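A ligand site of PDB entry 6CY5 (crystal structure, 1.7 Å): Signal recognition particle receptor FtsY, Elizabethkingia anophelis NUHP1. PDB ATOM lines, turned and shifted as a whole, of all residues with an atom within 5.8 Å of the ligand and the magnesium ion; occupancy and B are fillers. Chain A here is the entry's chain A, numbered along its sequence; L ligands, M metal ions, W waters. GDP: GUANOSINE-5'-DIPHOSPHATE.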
ATOM      1  N   VAL A 131     -32.606   3.737  27.162  1.00  0.00           N
ATOM      2  CA  VAL A 131     -33.406   4.089  28.324  1.00  0.00           C
ATOM      3  C   VAL A 131     -32.667   5.121  29.166  1.00  0.00           C
ATOM      4  O   VAL A 131     -31.432   5.176  29.160  1.00  0.00           O
ATOM      5  CB  VAL A 131     -33.713   2.807  29.120  1.00  0.00           C
ATOM      6  CG1 VAL A 131     -34.480   3.099  30.360  1.00  0.00           C
ATOM      7  CG2 VAL A 131     -34.516   1.842  28.244  1.00  0.00           C
ATOM      8  N   ASN A 132     -33.408   5.952  29.907  1.00  0.00           N
ATOM      9  CA  ASN A 132     -32.803   6.932  30.780  1.00  0.00           C
ATOM     10  C   ASN A 132     -31.821   6.284  31.753  1.00  0.00           C
ATOM     11  O   ASN A 132     -32.114   5.249  32.359  1.00  0.00           O
ATOM     12  CB  ASN A 132     -33.890   7.667  31.571  1.00  0.00           C
ATOM     13  CG  ASN A 132     -33.328   8.811  32.412  1.00  0.00           C
ATOM     14  OD1 ASN A 132     -33.121   9.905  31.897  1.00  0.00           O
ATOM     15  ND2 ASN A 132     -33.110   8.557  33.705  1.00  0.00           N
ATOM     16  N   GLY A 133     -30.661   6.917  31.910  1.00  0.00           N
ATOM     17  CA  GLY A 133     -29.673   6.513  32.883  1.00  0.00           C
ATOM     18  C   GLY A 133     -28.563   5.634  32.345  1.00  0.00           C
ATOM     19  O   GLY A 133     -27.599   5.385  33.077  1.00  0.00           O
ATOM     20  N   VAL A 134     -28.653   5.170  31.093  1.00  0.00           N
ATOM     21  CA  VAL A 134     -27.633   4.249  30.598  1.00  0.00           C
ATOM     22  C   VAL A 134     -26.360   4.962  30.175  1.00  0.00           C
ATOM     23  O   VAL A 134     -25.318   4.305  30.042  1.00  0.00           O
ATOM     24  CB  VAL A 134     -28.122   3.393  29.415  1.00  0.00           C
ATOM     25  CG1 VAL A 134     -29.267   2.497  29.844  1.00  0.00           C
ATOM     26  CG2 VAL A 134     -28.521   4.262  28.210  1.00  0.00           C
ATOM     27  N   GLY A 135     -26.418   6.274  29.931  1.00  0.00           N
ATOM     28  CA  GLY A 135     -25.268   7.036  29.480  1.00  0.00           C
ATOM     29  C   GLY A 135     -25.366   7.604  28.075  1.00  0.00           C
ATOM     30  O   GLY A 135     -24.326   7.851  27.445  1.00  0.00           O
ATOM     31  N   LYS A 136     -26.581   7.823  27.569  1.00  0.00           N
ATOM     32  CA  LYS A 136     -26.759   8.367  26.216  1.00  0.00           C
ATOM     33  C   LYS A 136     -26.088   9.715  26.059  1.00  0.00           C
ATOM     34  O   LYS A 136     -25.290   9.922  25.131  1.00  0.00           O
ATOM     35  CB  LYS A 136     -28.252   8.513  25.887  1.00  0.00           C
ATOM     36  CG  LYS A 136     -29.007   7.202  25.705  1.00  0.00           C
ATOM     37  CD  LYS A 136     -30.513   7.461  25.493  1.00  0.00           C
ATOM     38  CE  LYS A 136     -31.182   7.996  26.772  1.00  0.00           C
ATOM     39  NZ  LYS A 136     -32.668   8.229  26.602  1.00  0.00           N
ATOM     40  N   THR A 137     -26.436  10.668  26.924  1.00  0.00           N
ATOM     41  CA  THR A 137     -25.970  12.033  26.733  1.00  0.00           C
ATOM     42  C   THR A 137     -24.462  12.123  26.940  1.00  0.00           C
ATOM     43  O   THR A 137     -23.758  12.800  26.180  1.00  0.00           O
ATOM     44  CB  THR A 137     -26.747  12.960  27.682  1.00  0.00           C
ATOM     45  OG1 THR A 137     -28.156  12.807  27.423  1.00  0.00           O
ATOM     46  CG2 THR A 137     -26.330  14.428  27.487  1.00  0.00           C
ATOM     47  N   THR A 138     -23.947  11.376  27.937  1.00  0.00           N
ATOM     48  CA  THR A 138     -22.503  11.256  28.112  1.00  0.00           C
ATOM     49  C   THR A 138     -21.842  10.701  26.869  1.00  0.00           C
ATOM     50  O   THR A 138     -20.791  11.188  26.430  1.00  0.00           O
ATOM     51  CB  THR A 138     -22.223  10.353  29.308  1.00  0.00           C
ATOM     52  OG1 THR A 138     -22.800  10.931  30.486  1.00  0.00           O
ATOM     53  CG2 THR A 138     -20.705  10.174  29.492  1.00  0.00           C
ATOM     54  N   THR A 139     -22.428   9.648  26.297  1.00  0.00           N
ATOM     55  CA  THR A 139     -21.856   9.052  25.097  1.00  0.00           C
ATOM     56  C   THR A 139     -21.863  10.035  23.935  1.00  0.00           C
ATOM     57  O   THR A 139     -20.906  10.099  23.151  1.00  0.00           O
ATOM     58  CB  THR A 139     -22.610   7.765  24.768  1.00  0.00           C
ATOM     59  OG1 THR A 139     -22.448   6.851  25.866  1.00  0.00           O
ATOM     60  CG2 THR A 139     -22.072   7.106  23.473  1.00  0.00           C
ATOM     61  N   LYS A 142     -18.909  12.228  24.406  1.00  0.00           N
ATOM     62  CA  LYS A 142     -17.704  11.488  24.021  1.00  0.00           C
ATOM     63  C   LYS A 142     -17.591  11.374  22.502  1.00  0.00           C
ATOM     64  O   LYS A 142     -16.498  11.515  21.942  1.00  0.00           O
ATOM     65  CB  LYS A 142     -17.727  10.083  24.642  1.00  0.00           C
ATOM     66  CG  LYS A 142     -17.569  10.033  26.160  1.00  0.00           C
ATOM     67  CD  LYS A 142     -17.855   8.599  26.645  1.00  0.00           C
ATOM     68  CE  LYS A 142     -17.551   8.393  28.128  1.00  0.00           C
ATOM     69  NZ  LYS A 142     -17.761   6.924  28.473  1.00  0.00           N
ATOM     70  N   ASP A 160     -34.161  15.074  23.268  1.00  0.00           N
ATOM     71  CA  ASP A 160     -34.698  14.542  24.522  1.00  0.00           C
ATOM     72  C   ASP A 160     -35.302  15.742  25.243  1.00  0.00           C
ATOM     73  O   ASP A 160     -34.584  16.538  25.853  1.00  0.00           O
ATOM     74  CB  ASP A 160     -33.586  13.877  25.341  1.00  0.00           C
ATOM     75  CG  ASP A 160     -34.097  13.176  26.601  1.00  0.00           C
ATOM     76  OD1 ASP A 160     -35.268  13.365  26.965  1.00  0.00           O
ATOM     77  OD2 ASP A 160     -33.301  12.424  27.212  1.00  0.00           O
ATOM     78  N   ALA A 166     -32.868  17.406  30.762  1.00  0.00           N
ATOM     79  CA  ALA A 166     -32.286  16.724  29.612  1.00  0.00           C
ATOM     80  C   ALA A 166     -31.603  17.697  28.667  1.00  0.00           C
ATOM     81  O   ALA A 166     -30.454  17.483  28.253  1.00  0.00           O
ATOM     82  CB  ALA A 166     -33.350  15.918  28.858  1.00  0.00           C
ATOM     83  N   GLN A 169     -28.489  19.143  30.171  1.00  0.00           N
ATOM     84  CA  GLN A 169     -27.355  18.224  30.213  1.00  0.00           C
ATOM     85  C   GLN A 169     -26.631  18.171  28.872  1.00  0.00           C
ATOM     86  O   GLN A 169     -25.399  18.104  28.827  1.00  0.00           O
ATOM     87  CB  GLN A 169     -27.835  16.826  30.637  1.00  0.00           C
ATOM     88  CG  GLN A 169     -28.185  16.791  32.127  1.00  0.00           C
ATOM     89  CD  GLN A 169     -29.166  15.693  32.528  1.00  0.00           C
ATOM     90  OE1 GLN A 169     -29.630  14.895  31.708  1.00  0.00           O
ATOM     91  NE2 GLN A 169     -29.513  15.661  33.820  1.00  0.00           N
ATOM     92  N   TRP A 173     -22.687  19.361  27.840  1.00  0.00           N
ATOM     93  CA  TRP A 173     -21.696  18.627  27.067  1.00  0.00           C
ATOM     94  C   TRP A 173     -21.263  19.418  25.840  1.00  0.00           C
ATOM     95  O   TRP A 173     -20.088  19.373  25.449  1.00  0.00           O
ATOM     96  CB  TRP A 173     -22.218  17.248  26.664  1.00  0.00           C
ATOM     97  CG  TRP A 173     -21.864  16.230  27.687  1.00  0.00           C
ATOM     98  CD1 TRP A 173     -22.695  15.691  28.641  1.00  0.00           C
ATOM     99  CD2 TRP A 173     -20.574  15.661  27.926  1.00  0.00           C
ATOM    100  NE1 TRP A 173     -22.000  14.815  29.428  1.00  0.00           N
ATOM    101  CE2 TRP A 173     -20.694  14.781  29.013  1.00  0.00           C
ATOM    102  CE3 TRP A 173     -19.326  15.809  27.305  1.00  0.00           C
ATOM    103  CZ2 TRP A 173     -19.614  14.039  29.503  1.00  0.00           C
ATOM    104  CZ3 TRP A 173     -18.245  15.067  27.795  1.00  0.00           C
ATOM    105  CH2 TRP A 173     -18.403  14.185  28.879  1.00  0.00           C
ATOM    106  N   ASP A 212     -29.842  13.467  20.469  1.00  0.00           N
ATOM    107  CA  ASP A 212     -30.207  12.855  21.742  1.00  0.00           C
ATOM    108  C   ASP A 212     -31.710  12.584  21.772  1.00  0.00           C
ATOM    109  O   ASP A 212     -32.497  13.342  21.214  1.00  0.00           O
ATOM    110  CB  ASP A 212     -29.805  13.783  22.892  1.00  0.00           C
ATOM    111  CG  ASP A 212     -29.514  13.060  24.202  1.00  0.00           C
ATOM    112  OD1 ASP A 212     -29.859  11.873  24.353  1.00  0.00           O
ATOM    113  OD2 ASP A 212     -28.923  13.714  25.091  1.00  0.00           O
ATOM    114  N   THR A 213     -32.121  11.473  22.408  1.00  0.00           N
ATOM    115  CA  THR A 213     -33.536  11.120  22.457  1.00  0.00           C
ATOM    116  C   THR A 213     -33.902  10.598  23.837  1.00  0.00           C
ATOM    117  O   THR A 213     -33.053  10.139  24.612  1.00  0.00           O
ATOM    118  CB  THR A 213     -33.902  10.037  21.425  1.00  0.00           C
ATOM    119  OG1 THR A 213     -33.218   8.826  21.753  1.00  0.00           O
ATOM    120  CG2 THR A 213     -33.542  10.480  20.002  1.00  0.00           C
ATOM    121  N   THR A 276     -21.805   0.906  28.018  1.00  0.00           N
ATOM    122  CA  THR A 276     -21.135   1.871  28.887  1.00  0.00           C
ATOM    123  C   THR A 276     -20.855   1.282  30.269  1.00  0.00           C
ATOM    124  O   THR A 276     -21.308   0.198  30.622  1.00  0.00           O
ATOM    125  CB  THR A 276     -21.999   3.112  29.067  1.00  0.00           C
ATOM    126  OG1 THR A 276     -23.230   2.714  29.687  1.00  0.00           O
ATOM    127  CG2 THR A 276     -22.294   3.786  27.729  1.00  0.00           C
ATOM    128  N   LYS A 277     -20.115   2.069  31.061  1.00  0.00           N
ATOM    129  CA  LYS A 277     -19.949   1.833  32.501  1.00  0.00           C
ATOM    130  C   LYS A 277     -19.232   0.533  32.798  1.00  0.00           C
ATOM    131  O   LYS A 277     -19.440  -0.080  33.858  1.00  0.00           O
ATOM    132  CB  LYS A 277     -21.295   1.890  33.242  1.00  0.00           C
ATOM    133  CG  LYS A 277     -22.098   3.139  32.917  1.00  0.00           C
ATOM    134  CD  LYS A 277     -23.174   3.373  33.972  1.00  0.00           C
ATOM    135  CE  LYS A 277     -24.243   4.318  33.448  1.00  0.00           C
ATOM    136  NZ  LYS A 277     -25.300   4.517  34.489  1.00  0.00           N
ATOM    137  N   LEU A 278     -18.354   0.095  31.901  1.00  0.00           N
ATOM    138  CA  LEU A 278     -17.570  -1.108  32.175  1.00  0.00           C
ATOM    139  C   LEU A 278     -16.549  -0.896  33.279  1.00  0.00           C
ATOM    140  O   LEU A 278     -16.249  -1.824  34.034  1.00  0.00           O
ATOM    141  CB  LEU A 278     -16.878  -1.597  30.901  1.00  0.00           C
ATOM    142  CG  LEU A 278     -17.857  -1.962  29.786  1.00  0.00           C
ATOM    143  CD1 LEU A 278     -17.064  -2.455  28.582  1.00  0.00           C
ATOM    144  CD2 LEU A 278     -18.800  -3.060  30.292  1.00  0.00           C
ATOM    145  N   ASP A 279     -16.041   0.329  33.412  1.00  0.00           N
ATOM    146  CA  ASP A 279     -15.007   0.644  34.398  1.00  0.00           C
ATOM    147  C   ASP A 279     -15.567   0.555  35.812  1.00  0.00           C
ATOM    148  O   ASP A 279     -16.639   1.103  36.094  1.00  0.00           O
ATOM    149  CB  ASP A 279     -14.468   2.044  34.137  1.00  0.00           C
ATOM    150  CG  ASP A 279     -15.589   3.084  34.072  1.00  0.00           C
ATOM    151  OD1 ASP A 279     -16.481   2.960  33.197  1.00  0.00           O
ATOM    152  OD2 ASP A 279     -15.576   4.016  34.918  1.00  0.00           O
ATOM    153  N   GLY A 302     -17.839   2.117  26.735  1.00  0.00           N
ATOM    154  CA  GLY A 302     -17.549   3.221  27.627  1.00  0.00           C
ATOM    155  C   GLY A 302     -16.796   2.712  28.841  1.00  0.00           C
ATOM    156  O   GLY A 302     -17.190   1.720  29.462  1.00  0.00           O
ATOM    157  N   VAL A 303     -15.708   3.408  29.174  1.00  0.00           N
ATOM    158  CA  VAL A 303     -14.838   3.019  30.282  1.00  0.00           C
ATOM    159  C   VAL A 303     -14.573   4.188  31.210  1.00  0.00           C
ATOM    160  O   VAL A 303     -13.494   4.275  31.814  1.00  0.00           O
ATOM    161  CB  VAL A 303     -13.506   2.448  29.749  1.00  0.00           C
ATOM    162  CG1 VAL A 303     -13.714   1.126  29.055  1.00  0.00           C
ATOM    163  CG2 VAL A 303     -12.850   3.448  28.787  1.00  0.00           C
ATOM    164  N   GLY A 304     -15.529   5.093  31.355  1.00  0.00           N
ATOM    165  CA  GLY A 304     -15.349   6.158  32.337  1.00  0.00           C
ATOM    166  C   GLY A 304     -16.253   7.346  32.105  1.00  0.00           C
ATOM    167  O   GLY A 304     -17.044   7.395  31.178  1.00  0.00           O
ATOM    168  N   GLU A 305     -16.106   8.328  33.000  1.00  0.00           N
ATOM    169  CA  GLU A 305     -16.951   9.518  32.989  1.00  0.00           C
ATOM    170  C   GLU A 305     -16.443  10.623  32.079  1.00  0.00           C
ATOM    171  O   GLU A 305     -17.204  11.564  31.799  1.00  0.00           O
ATOM    172  CB  GLU A 305     -17.070  10.088  34.408  1.00  0.00           C
ATOM    173  CG  GLU A 305     -17.727   9.159  35.403  1.00  0.00           C
ATOM    174  CD  GLU A 305     -17.497   9.648  36.824  1.00  0.00           C
ATOM    175  OE1 GLU A 305     -16.554  10.443  37.033  1.00  0.00           O
ATOM    176  OE2 GLU A 305     -18.242   9.234  37.738  1.00  0.00           O
ATOM    177  N   ASP A 309     -13.255   8.754  27.480  1.00  0.00           N
ATOM    178  CA  ASP A 309     -13.449   7.371  27.944  1.00  0.00           C
ATOM    179  C   ASP A 309     -14.443   6.594  27.075  1.00  0.00           C
ATOM    180  O   ASP A 309     -15.402   5.983  27.536  1.00  0.00           O
ATOM    181  CB  ASP A 309     -13.872   7.384  29.412  1.00  0.00           C
ATOM    182  CG  ASP A 309     -12.816   7.972  30.334  1.00  0.00           C
ATOM    183  OD1 ASP A 309     -11.606   7.948  29.974  1.00  0.00           O
ATOM    184  OD2 ASP A 309     -13.177   8.450  31.435  1.00  0.00           O
HETATM  185  PB  GDP L   1     -28.698   9.179  29.956  1.00  0.00           P
HETATM  186  O1B GDP L   1     -29.903   9.353  30.854  1.00  0.00           O
HETATM  187  O2B GDP L   1     -28.812   7.825  29.274  1.00  0.00           O
HETATM  188  O3B GDP L   1     -28.551  10.307  28.983  1.00  0.00           O
HETATM  189  O3A GDP L   1     -27.384   9.071  30.873  1.00  0.00           O
HETATM  190  PA  GDP L   1     -26.310  10.202  31.221  1.00  0.00           P
HETATM  191  O1A GDP L   1     -26.982  11.398  31.887  1.00  0.00           O
HETATM  192  O2A GDP L   1     -25.473  10.601  30.047  1.00  0.00           O
HETATM  193  O5' GDP L   1     -25.354   9.404  32.244  1.00  0.00           O
HETATM  194  C5' GDP L   1     -25.812   8.916  33.496  1.00  0.00           C
HETATM  195  C4' GDP L   1     -24.577   8.644  34.339  1.00  0.00           C
HETATM  196  O4' GDP L   1     -23.826   7.571  33.763  1.00  0.00           O
HETATM  197  C3' GDP L   1     -23.640   9.843  34.428  1.00  0.00           C
HETATM  198  O3' GDP L   1     -23.287  10.038  35.806  1.00  0.00           O
HETATM  199  C2' GDP L   1     -22.379   9.436  33.693  1.00  0.00           C
HETATM  200  O2' GDP L   1     -21.180   9.948  34.283  1.00  0.00           O
HETATM  201  C1' GDP L   1     -22.447   7.920  33.815  1.00  0.00           C
HETATM  202  N9  GDP L   1     -21.715   7.232  32.743  1.00  0.00           N
HETATM  203  C8  GDP L   1     -22.030   7.191  31.413  1.00  0.00           C
HETATM  204  N7  GDP L   1     -21.097   6.459  30.741  1.00  0.00           N
HETATM  205  C5  GDP L   1     -20.205   6.007  31.667  1.00  0.00           C
HETATM  206  C6  GDP L   1     -19.003   5.156  31.659  1.00  0.00           C
HETATM  207  O6  GDP L   1     -18.571   4.680  30.600  1.00  0.00           O
HETATM  208  N1  GDP L   1     -18.354   4.949  32.825  1.00  0.00           N
HETATM  209  C2  GDP L   1     -18.796   5.455  33.998  1.00  0.00           C
HETATM  210  N2  GDP L   1     -18.101   5.197  35.142  1.00  0.00           N
HETATM  211  N3  GDP L   1     -19.905   6.231  34.093  1.00  0.00           N
HETATM  212  C4  GDP L   1     -20.627   6.525  32.969  1.00  0.00           C
HETATM  213 MG    MG M   1     -29.618  12.017  28.642  1.00  0.00          MG
HETATM  214  O   HOH W   1     -18.194   6.300  37.617  1.00  0.00           O
HETATM  215  O   HOH W   2     -25.286  10.929  37.136  1.00  0.00           O
HETATM  216  O   HOH W   3     -28.783  12.844  30.287  1.00  0.00           O
HETATM  217  O   HOH W   4     -29.595  10.251  33.365  1.00  0.00           O
HETATM  218  O   HOH W   5     -31.254  11.331  29.766  1.00  0.00           O
HETATM  219  O   HOH W   6     -20.404   6.662  27.900  1.00  0.00           O
HETATM  220  O   HOH W   7     -30.594  11.328  26.866  1.00  0.00           O
HETATM  221  O   HOH W   8     -30.856  13.763  28.459  1.00  0.00           O
HETATM  222  O   HOH W   9     -25.792  13.044  33.654  1.00  0.00           O
HETATM  223  O   HOH W  10     -21.421   5.699  36.694  1.00  0.00           O
HETATM  224  O   HOH W  11     -20.639   9.517  36.881  1.00  0.00           O
HETATM  225  O   HOH W  12     -19.741  11.776  32.783  1.00  0.00           O
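Water W3 lies within hydrogen-bond range of the side-chain amide oxygen of Gln 169 and an oxygen (O1A) of the ligand. Water W7 lies within hydrogen-bond range of OD1 of Asp 212 (2.7 Å) and OD2 of Asp 160 (2.9 Å). Water W5 lies within hydrogen-bond range of an oxygen (O1B) of the ligand, the side-chain amide oxygen of Asn 132 and the side-chain carboxylate of Asp 160. Water W11 lies within hydrogen-bond range of OE2 of Glu 305 (2.6 Å) and O2' of the ligand (2.7 Å). Water W12 bridges O of Glu 305 and O2' of the ligand. Water W6 lies within hydrogen-bond range of NZ of Lys 142 (2.7 Å), OG1 of Thr 139 (2.9 Å) and N7 of the ligand (2.9 Å).
N of Thr 137 is in hydrogen-bond range of O2A of the ligand (3.3 Å). The backbone NH (N) of Thr 138 is in hydrogen-bond range of an oxygen (O2A) of the ligand (2.7 Å). OG1 of Thr 138 lies within hydrogen-bond range of O2A of the ligand. OD1 of Asp 279 sits at hydrogen-bond distance from N1 of the ligand (2.8 Å). N of Gly 133 lies within hydrogen-bond range of O1B of the ligand (2.8 Å). The backbone NH of Lys 136 is in hydrogen-bond range of an oxygen (O2B) of the ligand (2.8 Å). The backbone NH (N) of Gly 135 sits at hydrogen-bond distance from an oxygen (O2B) of the ligand, 2.9 Å away. O6 of the ligand lies within hydrogen-bond range of N of Gly 304 (3.2 Å). A nitrogen (N1) of the ligand sits close to the backbone carbonyl oxygen (O) of Gly 304 (3.2 Å). An oxygen (O6) of the ligand lies within hydrogen-bond range of the backbone NH of Lys 277, 3.1 Å away. An oxygen (O4') of the ligand lies close to the side-chain amino group (NZ) of Lys 277, 3.5 Å away. The side-chain amino group of Lys 142 lies within hydrogen-bond range of an oxygen (O6) of the ligand (3.2 Å). N of Val 134 sits at hydrogen-bond distance from O2B of the ligand (3.2 Å). OD1 of Asn 132 sits close to O1B of the ligand (3.4 Å). The backbone NH of Val 303 lies within hydrogen-bond range of an oxygen (O6) of the ligand (3.4 Å).
The side-chain hydroxyl of Thr 137 sits close to the side-chain carboxylate of Asp 212, 2.6 Å away. N of Gly 304 sits at hydrogen-bond distance from OD1 of Asp 279, 3.0 Å away. The backbone carbonyl oxygen of Gly 133 is in hydrogen-bond range of the side-chain amino group of Lys 277, at 2.8 Å. NZ of Lys 136 sits at hydrogen-bond distance from O of Thr 213, 2.8 Å away. The backbone carbonyl oxygen of Gly 304 sits at hydrogen-bond distance from the side-chain amino group of Lys 142, 2.8 Å away. NZ of Lys 142 is in hydrogen-bond range of O of Asp 309, 2.7 Å away. The backbone NH of Val 303 is in hydrogen-bond range of the backbone carbonyl oxygen of Asp 309 (3.1 Å). The backbone NH (N) of Asp 160 sits at hydrogen-bond distance from the backbone carbonyl oxygen (O) of Asp 212 (3.2 Å).
The magnesium ion is bound by water W3 (2.0 Å), an oxygen (O3B) of the ligand (2.0 Å), the side-chain hydroxyl (OG1) of Thr 137 (2.1 Å), water W5 (2.1 Å), water W7 (2.1 Å) and water W8 (2.1 Å). The magnesium ion has six donor atoms within binding distance.
O of Gly 302 sits close to O6 of the ligand, 3.5 Å away. Merely in contact with the ligand: Glu 305 (3.7 Å), Val 131 (3.7 Å) and Thr 276 (3.8 Å). Hydrophobic or aromatic side chains that line the ligand: Val 134. 16 residues have an atom within 4 Å of the ligand: Val 131, Asn 132, Gly 133, Val 134, Gly 135, Lys 136, Thr 137, Thr 138, Lys 142, Thr 276, Lys 277, Asp 279, Gly 302, Val 303, Gly 304 and Glu 305. Along chain A the residues within 4 Å of the ligand span positions 131 to 305.
Merely in contact with the magnesium ion: Asp 160 (3.97 Å) and Asp 212 (3.997 Å). Three residues have an atom within 4 Å of the magnesium ion: Thr 137, Asp 160 and Asp 212. The nearest printed residue that does not touch the magnesium ion is Gln 169 (4.2 Å).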
